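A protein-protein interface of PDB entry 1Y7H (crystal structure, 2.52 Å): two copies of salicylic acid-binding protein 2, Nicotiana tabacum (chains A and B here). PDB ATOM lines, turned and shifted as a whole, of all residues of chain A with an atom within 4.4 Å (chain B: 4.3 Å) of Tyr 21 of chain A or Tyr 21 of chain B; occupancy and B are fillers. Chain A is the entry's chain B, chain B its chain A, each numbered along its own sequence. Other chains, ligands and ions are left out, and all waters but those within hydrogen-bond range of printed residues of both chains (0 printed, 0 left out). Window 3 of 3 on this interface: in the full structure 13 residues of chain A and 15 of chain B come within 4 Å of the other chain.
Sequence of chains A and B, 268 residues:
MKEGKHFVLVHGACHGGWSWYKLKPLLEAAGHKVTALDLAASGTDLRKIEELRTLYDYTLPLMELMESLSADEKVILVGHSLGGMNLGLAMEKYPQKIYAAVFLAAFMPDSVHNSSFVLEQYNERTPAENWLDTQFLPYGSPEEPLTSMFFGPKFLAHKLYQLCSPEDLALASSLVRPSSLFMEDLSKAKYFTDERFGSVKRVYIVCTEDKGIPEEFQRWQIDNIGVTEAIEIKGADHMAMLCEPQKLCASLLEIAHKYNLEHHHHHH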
ATOM      1  N   GLY A  17      -7.750  16.060  37.484  1.00  0.00           N
ATOM      2  CA  GLY A  17      -8.368  17.318  37.131  1.00  0.00           C
ATOM      3  C   GLY A  17      -8.287  17.655  35.662  1.00  0.00           C
ATOM      4  O   GLY A  17      -9.125  18.402  35.156  1.00  0.00           O
ATOM      5  N   TRP A  18      -7.277  17.130  34.971  1.00  0.00           N
ATOM      6  CA  TRP A  18      -7.136  17.401  33.543  1.00  0.00           C
ATOM      7  C   TRP A  18      -8.397  16.972  32.830  1.00  0.00           C
ATOM      8  O   TRP A  18      -8.847  17.626  31.904  1.00  0.00           O
ATOM      9  CB  TRP A  18      -5.935  16.657  32.953  1.00  0.00           C
ATOM     10  CG  TRP A  18      -5.850  15.223  33.317  1.00  0.00           C
ATOM     11  CD1 TRP A  18      -5.229  14.684  34.417  1.00  0.00           C
ATOM     12  CD2 TRP A  18      -6.394  14.120  32.583  1.00  0.00           C
ATOM     13  NE1 TRP A  18      -5.350  13.313  34.403  1.00  0.00           N
ATOM     14  CE2 TRP A  18      -6.058  12.939  33.290  1.00  0.00           C
ATOM     15  CE3 TRP A  18      -7.129  14.012  31.389  1.00  0.00           C
ATOM     16  CZ2 TRP A  18      -6.431  11.671  32.849  1.00  0.00           C
ATOM     17  CZ3 TRP A  18      -7.503  12.740  30.946  1.00  0.00           C
ATOM     18  CH2 TRP A  18      -7.150  11.587  31.678  1.00  0.00           C
ATOM     19  N   SER A  19      -8.956  15.860  33.285  1.00  0.00           N
ATOM     20  CA  SER A  19     -10.175  15.321  32.723  1.00  0.00           C
ATOM     21  C   SER A  19     -11.206  16.398  32.379  1.00  0.00           C
ATOM     22  O   SER A  19     -11.952  16.249  31.419  1.00  0.00           O
ATOM     23  CB  SER A  19     -10.789  14.320  33.702  1.00  0.00           C
ATOM     24  OG  SER A  19     -11.492  13.309  33.015  1.00  0.00           O
ATOM     25  N   TRP A  20     -11.252  17.495  33.127  1.00  0.00           N
ATOM     26  CA  TRP A  20     -12.261  18.534  32.849  1.00  0.00           C
ATOM     27  C   TRP A  20     -11.795  19.680  31.938  1.00  0.00           C
ATOM     28  O   TRP A  20     -12.441  20.731  31.863  1.00  0.00           O
ATOM     29  CB  TRP A  20     -12.775  19.131  34.167  1.00  0.00           C
ATOM     30  CG  TRP A  20     -13.170  18.120  35.196  1.00  0.00           C
ATOM     31  CD1 TRP A  20     -12.356  17.532  36.100  1.00  0.00           C
ATOM     32  CD2 TRP A  20     -14.479  17.567  35.413  1.00  0.00           C
ATOM     33  NE1 TRP A  20     -13.066  16.640  36.878  1.00  0.00           N
ATOM     34  CE2 TRP A  20     -14.373  16.643  36.474  1.00  0.00           C
ATOM     35  CE3 TRP A  20     -15.731  17.759  34.811  1.00  0.00           C
ATOM     36  CZ2 TRP A  20     -15.456  15.914  36.949  1.00  0.00           C
ATOM     37  CZ3 TRP A  20     -16.818  17.027  35.286  1.00  0.00           C
ATOM     38  CH2 TRP A  20     -16.669  16.116  36.347  1.00  0.00           C
ATOM     39  N   TYR A  21     -10.687  19.456  31.239  1.00  0.00           N
ATOM     40  CA  TYR A  21     -10.087  20.447  30.348  1.00  0.00           C
ATOM     41  C   TYR A  21     -10.926  21.012  29.179  1.00  0.00           C
ATOM     42  O   TYR A  21     -10.603  22.072  28.639  1.00  0.00           O
ATOM     43  CB  TYR A  21      -8.758  19.890  29.818  1.00  0.00           C
ATOM     44  CG  TYR A  21      -8.811  19.198  28.471  1.00  0.00           C
ATOM     45  CD1 TYR A  21      -8.769  19.943  27.292  1.00  0.00           C
ATOM     46  CD2 TYR A  21      -8.835  17.792  28.373  1.00  0.00           C
ATOM     47  CE1 TYR A  21      -8.738  19.321  26.052  1.00  0.00           C
ATOM     48  CE2 TYR A  21      -8.809  17.150  27.121  1.00  0.00           C
ATOM     49  CZ  TYR A  21      -8.757  17.931  25.962  1.00  0.00           C
ATOM     50  OH  TYR A  21      -8.729  17.358  24.704  1.00  0.00           O
ATOM     51  N   LYS A  22     -11.985  20.312  28.783  1.00  0.00           N
ATOM     52  CA  LYS A  22     -12.834  20.776  27.690  1.00  0.00           C
ATOM     53  C   LYS A  22     -14.081  21.479  28.216  1.00  0.00           C
ATOM     54  O   LYS A  22     -14.698  22.265  27.504  1.00  0.00           O
ATOM     55  CB  LYS A  22     -13.256  19.607  26.812  1.00  0.00           C
ATOM     56  CG  LYS A  22     -12.217  19.138  25.831  1.00  0.00           C
ATOM     57  CD  LYS A  22     -12.826  18.079  24.891  1.00  0.00           C
ATOM     58  CE  LYS A  22     -11.771  17.382  24.032  1.00  0.00           C
ATOM     59  NZ  LYS A  22     -12.343  16.164  23.410  1.00  0.00           N
ATOM     60  N   LEU A  23     -14.432  21.188  29.470  1.00  0.00           N
ATOM     61  CA  LEU A  23     -15.588  21.772  30.130  1.00  0.00           C
ATOM     62  C   LEU A  23     -15.254  23.068  30.873  1.00  0.00           C
ATOM     63  O   LEU A  23     -16.000  24.051  30.808  1.00  0.00           O
ATOM     64  CB  LEU A  23     -16.184  20.772  31.123  1.00  0.00           C
ATOM     65  CG  LEU A  23     -17.361  21.321  31.951  1.00  0.00           C
ATOM     66  CD1 LEU A  23     -18.544  21.634  31.036  1.00  0.00           C
ATOM     67  CD2 LEU A  23     -17.752  20.307  33.020  1.00  0.00           C
ATOM     68  N   PRO A  25     -13.247  25.696  30.379  1.00  0.00           N
ATOM     69  CA  PRO A  25     -13.320  26.968  29.643  1.00  0.00           C
ATOM     70  C   PRO A  25     -14.756  27.445  29.378  1.00  0.00           C
ATOM     71  O   PRO A  25     -15.040  28.646  29.370  1.00  0.00           O
ATOM     72  CB  PRO A  25     -12.577  26.666  28.337  1.00  0.00           C
ATOM     73  CG  PRO A  25     -11.781  25.380  28.648  1.00  0.00           C
ATOM     74  CD  PRO A  25     -12.723  24.627  29.512  1.00  0.00           C
ATOM     75  N   GLU A 167      -7.774  11.477  19.904  1.00  0.00           N
ATOM     76  CA  GLU A 167      -6.852  12.385  20.582  1.00  0.00           C
ATOM     77  C   GLU A 167      -7.109  12.234  22.092  1.00  0.00           C
ATOM     78  O   GLU A 167      -6.184  12.078  22.905  1.00  0.00           O
ATOM     79  CB  GLU A 167      -7.103  13.834  20.122  1.00  0.00           C
ATOM     80  CG  GLU A 167      -6.981  14.106  18.583  1.00  0.00           C
ATOM     81  CD  GLU A 167      -8.091  13.459  17.721  1.00  0.00           C
ATOM     82  OE1 GLU A 167      -9.258  13.413  18.158  1.00  0.00           O
ATOM     83  OE2 GLU A 167      -7.799  13.014  16.589  1.00  0.00           O
ATOM     84  N   ASP A 168      -8.390  12.252  22.446  1.00  0.00           N
ATOM     85  CA  ASP A 168      -8.834  12.099  23.830  1.00  0.00           C
ATOM     86  C   ASP A 168      -8.377  10.751  24.427  1.00  0.00           C
ATOM     87  O   ASP A 168      -7.974  10.686  25.596  1.00  0.00           O
ATOM     88  CB  ASP A 168     -10.363  12.221  23.885  1.00  0.00           C
ATOM     89  CG  ASP A 168     -10.857  13.548  23.324  1.00  0.00           C
ATOM     90  OD1 ASP A 168     -12.031  13.624  22.888  1.00  0.00           O
ATOM     91  OD2 ASP A 168     -10.062  14.518  23.327  1.00  0.00           O
ATOM     92  N   ALA A 170      -5.739   8.967  23.462  1.00  0.00           N
ATOM     93  CA  ALA A 170      -4.283   9.034  23.581  1.00  0.00           C
ATOM     94  C   ALA A 170      -3.882   9.854  24.809  1.00  0.00           C
ATOM     95  O   ALA A 170      -2.906   9.548  25.474  1.00  0.00           O
ATOM     96  CB  ALA A 170      -3.683   9.655  22.317  1.00  0.00           C
ATOM     97  N   LEU A 171      -4.635  10.907  25.097  1.00  0.00           N
ATOM     98  CA  LEU A 171      -4.342  11.744  26.252  1.00  0.00           C
ATOM     99  C   LEU A 171      -4.538  10.919  27.517  1.00  0.00           C
ATOM    100  O   LEU A 171      -3.625  10.764  28.327  1.00  0.00           O
ATOM    101  CB  LEU A 171      -5.286  12.938  26.269  1.00  0.00           C
ATOM    102  CG  LEU A 171      -5.274  13.861  27.482  1.00  0.00           C
ATOM    103  CD1 LEU A 171      -3.879  14.460  27.701  1.00  0.00           C
ATOM    104  CD2 LEU A 171      -6.295  14.963  27.252  1.00  0.00           C
ATOM    105  N   LEU A 242     -15.723  14.823  27.751  1.00  0.00           N
ATOM    106  CA  LEU A 242     -14.792  14.826  26.633  1.00  0.00           C
ATOM    107  C   LEU A 242     -15.511  14.681  25.293  1.00  0.00           C
ATOM    108  O   LEU A 242     -15.140  15.331  24.318  1.00  0.00           O
ATOM    109  CB  LEU A 242     -13.781  13.702  26.792  1.00  0.00           C
ATOM    110  CG  LEU A 242     -12.896  13.793  28.032  1.00  0.00           C
ATOM    111  CD1 LEU A 242     -12.101  12.522  28.106  1.00  0.00           C
ATOM    112  CD2 LEU A 242     -11.978  14.995  27.978  1.00  0.00           C
ATOM    113  N   TRP B  18       1.955  13.721  27.540  1.00  0.00           N
ATOM    114  CA  TRP B  18       0.573  14.041  27.196  1.00  0.00           C
ATOM    115  C   TRP B  18       0.468  15.172  26.191  1.00  0.00           C
ATOM    116  O   TRP B  18      -0.538  15.297  25.493  1.00  0.00           O
ATOM    117  CB  TRP B  18      -0.232  14.430  28.445  1.00  0.00           C
ATOM    118  CG  TRP B  18       0.375  15.559  29.187  1.00  0.00           C
ATOM    119  CD1 TRP B  18       1.297  15.473  30.185  1.00  0.00           C
ATOM    120  CD2 TRP B  18       0.168  16.957  28.945  1.00  0.00           C
ATOM    121  NE1 TRP B  18       1.678  16.728  30.582  1.00  0.00           N
ATOM    122  CE2 TRP B  18       1.003  17.658  29.839  1.00  0.00           C
ATOM    123  CE3 TRP B  18      -0.645  17.684  28.061  1.00  0.00           C
ATOM    124  CZ2 TRP B  18       1.058  19.057  29.873  1.00  0.00           C
ATOM    125  CZ3 TRP B  18      -0.590  19.079  28.097  1.00  0.00           C
ATOM    126  CH2 TRP B  18       0.258  19.748  28.999  1.00  0.00           C
ATOM    127  N   SER B  19       1.492  16.009  26.119  1.00  0.00           N
ATOM    128  CA  SER B  19       1.434  17.128  25.185  1.00  0.00           C
ATOM    129  C   SER B  19       1.358  16.667  23.718  1.00  0.00           C
ATOM    130  O   SER B  19       1.052  17.466  22.842  1.00  0.00           O
ATOM    131  CB  SER B  19       2.638  18.072  25.399  1.00  0.00           C
ATOM    132  OG  SER B  19       3.868  17.360  25.459  1.00  0.00           O
ATOM    133  N   TRP B  20       1.607  15.384  23.452  1.00  0.00           N
ATOM    134  CA  TRP B  20       1.576  14.885  22.078  1.00  0.00           C
ATOM    135  C   TRP B  20       0.278  14.174  21.735  1.00  0.00           C
ATOM    136  O   TRP B  20       0.180  13.496  20.701  1.00  0.00           O
ATOM    137  CB  TRP B  20       2.750  13.926  21.810  1.00  0.00           C
ATOM    138  CG  TRP B  20       4.124  14.500  22.121  1.00  0.00           C
ATOM    139  CD1 TRP B  20       4.853  14.294  23.254  1.00  0.00           C
ATOM    140  CD2 TRP B  20       4.921  15.359  21.288  1.00  0.00           C
ATOM    141  NE1 TRP B  20       6.059  14.957  23.184  1.00  0.00           N
ATOM    142  CE2 TRP B  20       6.132  15.613  21.983  1.00  0.00           C
ATOM    143  CE3 TRP B  20       4.744  15.923  20.019  1.00  0.00           C
ATOM    144  CZ2 TRP B  20       7.150  16.424  21.455  1.00  0.00           C
ATOM    145  CZ3 TRP B  20       5.761  16.728  19.499  1.00  0.00           C
ATOM    146  CH2 TRP B  20       6.946  16.960  20.213  1.00  0.00           C
ATOM    147  N   TYR B  21      -0.726  14.344  22.595  1.00  0.00           N
ATOM    148  CA  TYR B  21      -2.015  13.677  22.405  1.00  0.00           C
ATOM    149  C   TYR B  21      -2.697  14.005  21.067  1.00  0.00           C
ATOM    150  O   TYR B  21      -3.503  13.215  20.557  1.00  0.00           O
ATOM    151  CB  TYR B  21      -2.956  13.974  23.587  1.00  0.00           C
ATOM    152  CG  TYR B  21      -3.724  15.277  23.531  1.00  0.00           C
ATOM    153  CD1 TYR B  21      -5.073  15.300  23.161  1.00  0.00           C
ATOM    154  CD2 TYR B  21      -3.121  16.473  23.899  1.00  0.00           C
ATOM    155  CE1 TYR B  21      -5.805  16.485  23.165  1.00  0.00           C
ATOM    156  CE2 TYR B  21      -3.834  17.663  23.906  1.00  0.00           C
ATOM    157  CZ  TYR B  21      -5.178  17.669  23.540  1.00  0.00           C
ATOM    158  OH  TYR B  21      -5.884  18.855  23.547  1.00  0.00           O
ATOM    159  N   LYS B  22      -2.373  15.147  20.480  1.00  0.00           N
ATOM    160  CA  LYS B  22      -2.984  15.472  19.206  1.00  0.00           C
ATOM    161  C   LYS B  22      -2.182  14.892  18.061  1.00  0.00           C
ATOM    162  O   LYS B  22      -2.748  14.407  17.085  1.00  0.00           O
ATOM    163  CB  LYS B  22      -3.112  16.979  19.036  1.00  0.00           C
ATOM    164  CG  LYS B  22      -4.104  17.629  19.980  1.00  0.00           C
ATOM    165  CD  LYS B  22      -4.306  19.068  19.561  1.00  0.00           C
ATOM    166  CE  LYS B  22      -5.339  19.774  20.379  1.00  0.00           C
ATOM    167  NZ  LYS B  22      -5.576  21.129  19.816  1.00  0.00           N
ATOM    168  N   LEU B  23      -0.861  14.926  18.181  1.00  0.00           N
ATOM    169  CA  LEU B  23       0.000  14.400  17.116  1.00  0.00           C
ATOM    170  C   LEU B  23       0.097  12.868  17.096  1.00  0.00           C
ATOM    171  O   LEU B  23       0.150  12.256  16.027  1.00  0.00           O
ATOM    172  CB  LEU B  23       1.415  14.996  17.244  1.00  0.00           C
ATOM    173  CG  LEU B  23       2.498  14.633  16.224  1.00  0.00           C
ATOM    174  CD1 LEU B  23       2.220  15.371  14.921  1.00  0.00           C
ATOM    175  CD2 LEU B  23       3.880  15.022  16.761  1.00  0.00           C
ATOM    176  N   PRO B  25      -2.012  10.260  17.568  1.00  0.00           N
ATOM    177  CA  PRO B  25      -3.014   9.563  16.754  1.00  0.00           C
ATOM    178  C   PRO B  25      -2.751   9.764  15.270  1.00  0.00           C
ATOM    179  O   PRO B  25      -2.821   8.817  14.485  1.00  0.00           O
ATOM    180  CB  PRO B  25      -4.321  10.215  17.186  1.00  0.00           C
ATOM    181  CG  PRO B  25      -4.054  10.565  18.600  1.00  0.00           C
ATOM    182  CD  PRO B  25      -2.676  11.159  18.525  1.00  0.00           C
ATOM    183  N   GLU B 167      -9.080  25.378  25.740  1.00  0.00           N
ATOM    184  CA  GLU B 167      -9.072  24.025  26.263  1.00  0.00           C
ATOM    185  C   GLU B 167      -7.634  23.634  26.559  1.00  0.00           C
ATOM    186  O   GLU B 167      -7.297  23.275  27.686  1.00  0.00           O
ATOM    187  CB  GLU B 167      -9.677  23.056  25.247  1.00  0.00           C
ATOM    188  CG  GLU B 167     -11.153  23.277  24.971  1.00  0.00           C
ATOM    189  CD  GLU B 167     -11.465  24.651  24.360  1.00  0.00           C
ATOM    190  OE1 GLU B 167     -10.567  25.251  23.731  1.00  0.00           O
ATOM    191  OE2 GLU B 167     -12.613  25.123  24.504  1.00  0.00           O
ATOM    192  N   ASP B 168      -6.787  23.715  25.535  1.00  0.00           N
ATOM    193  CA  ASP B 168      -5.370  23.381  25.657  1.00  0.00           C
ATOM    194  C   ASP B 168      -4.719  24.126  26.827  1.00  0.00           C
ATOM    195  O   ASP B 168      -3.860  23.579  27.503  1.00  0.00           O
ATOM    196  CB  ASP B 168      -4.625  23.753  24.368  1.00  0.00           C
ATOM    197  CG  ASP B 168      -4.847  22.764  23.229  1.00  0.00           C
ATOM    198  OD1 ASP B 168      -4.579  23.165  22.073  1.00  0.00           O
ATOM    199  OD2 ASP B 168      -5.267  21.606  23.471  1.00  0.00           O
ATOM    200  N   ALA B 170      -6.235  25.102  29.489  1.00  0.00           N
ATOM    201  CA  ALA B 170      -6.805  24.567  30.712  1.00  0.00           C
ATOM    202  C   ALA B 170      -6.104  23.274  31.039  1.00  0.00           C
ATOM    203  O   ALA B 170      -5.800  23.004  32.201  1.00  0.00           O
ATOM    204  CB  ALA B 170      -8.281  24.317  30.528  1.00  0.00           C
ATOM    205  N   LEU B 171      -5.844  22.478  30.004  1.00  0.00           N
ATOM    206  CA  LEU B 171      -5.169  21.197  30.188  1.00  0.00           C
ATOM    207  C   LEU B 171      -3.813  21.417  30.864  1.00  0.00           C
ATOM    208  O   LEU B 171      -3.550  20.870  31.932  1.00  0.00           O
ATOM    209  CB  LEU B 171      -4.991  20.489  28.832  1.00  0.00           C
ATOM    210  CG  LEU B 171      -4.211  19.161  28.786  1.00  0.00           C
ATOM    211  CD1 LEU B 171      -4.922  18.103  29.609  1.00  0.00           C
ATOM    212  CD2 LEU B 171      -4.061  18.687  27.326  1.00  0.00           C
ATOM    213  N   LEU B 242      -0.085  21.200  19.423  1.00  0.00           N
ATOM    214  CA  LEU B 242      -1.419  21.448  19.945  1.00  0.00           C
ATOM    215  C   LEU B 242      -2.251  22.365  19.057  1.00  0.00           C
ATOM    216  O   LEU B 242      -3.455  22.151  18.888  1.00  0.00           O
ATOM    217  CB  LEU B 242      -1.317  22.039  21.347  1.00  0.00           C
ATOM    218  CG  LEU B 242      -0.487  21.215  22.336  1.00  0.00           C
ATOM    219  CD1 LEU B 242      -0.413  21.977  23.646  1.00  0.00           C
ATOM    220  CD2 LEU B 242      -1.093  19.845  22.543  1.00  0.00           C
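The side-chain hydroxyl of Tyr 21 of chain A is in hydrogen-bond range of the side-chain hydroxyl of Tyr 21 of chain B (3.4 Å).
OH of Tyr 21 of chain B is in hydrogen-bond range of OD2 of Asp 168 of chain B, 2.8 Å away.
OD2 of Asp 168 of chain A lies within hydrogen-bond range of OH of Tyr 21 of chain A.
Among the printed residues, pairs that only touch across the chains: Trp 18 of chain A with Leu 171 of chain B (3.8 Å), Tyr 21 of chain A with Glu 167 of chain B (3.4 Å), Tyr 21 of chain A with Ala 170 of chain B (3.7 Å), Tyr 21 of chain A with Leu 171 of chain B (3.8 Å), Pro 25 of chain A with Glu 167 of chain B (3.9 Å), Glu 167 of chain A with Tyr 21 of chain B (3.4 Å), Glu 167 of chain A with Pro 25 of chain B (3.9 Å), Ala 170 of chain A with Tyr 21 of chain B (3.98 Å), Ala 170 of chain A with Pro 25 of chain B (3.8 Å), Leu 171 of chain A with Trp 18 of chain B (3.7 Å) and Leu 171 of chain A with Tyr 21 of chain B (3.7 Å).
Of the printed residues of chain B, Trp 18 of chain A touches Leu 171 (3.8 Å).
Of the printed residues of chain B, Leu 171 of chain A touches Trp 18 (3.7 Å) and Tyr 21 (3.7 Å).
Printed residues of chain A within 4 Å of Trp 18 of chain B: Leu 171.
Of the printed residues of chain A, Tyr 21 of chain B touches Tyr 21 (3.4 Å), Glu 167 (3.4 Å), Ala 170 (3.98 Å) and Leu 171 (3.7 Å).
Printed residues of chain A within 4 Å of Glu 167 of chain B: Tyr 21 and Pro 25.
Of the printed residues of chain A, Leu 171 of chain B touches Trp 18 and Tyr 21.
The nearest printed residue of chain A that does not touch Tyr 21 of chain B is Asp 168 of chain A (4.6 Å).
Among the printed residues, 12 pairs touch across the chains.
Among the printed residues, no Asp or Glu carboxylate lies within 4 Å of a Lys or Arg side-chain nitrogen of the other chain.
Tyr 21 of chain B touches its own counterpart, Tyr 21 of chain A.
Tyr 21 of chain A touches Glu 167 of chain B, and with the chains exchanged Glu 167 of chain A touches Tyr 21 of chain B.
Tyr 21 of chain A touches Leu 171 of chain B, and with the chains exchanged Leu 171 of chain A touches Tyr 21 of chain B.
Pro 25 of chain A touches Glu 167 of chain B, and with the chains exchanged Glu 167 of chain A touches Pro 25 of chain B.
Of the 12 pairs that touch across the chains among the printed residues, 11 have their exchanged pair printed and touching as well.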
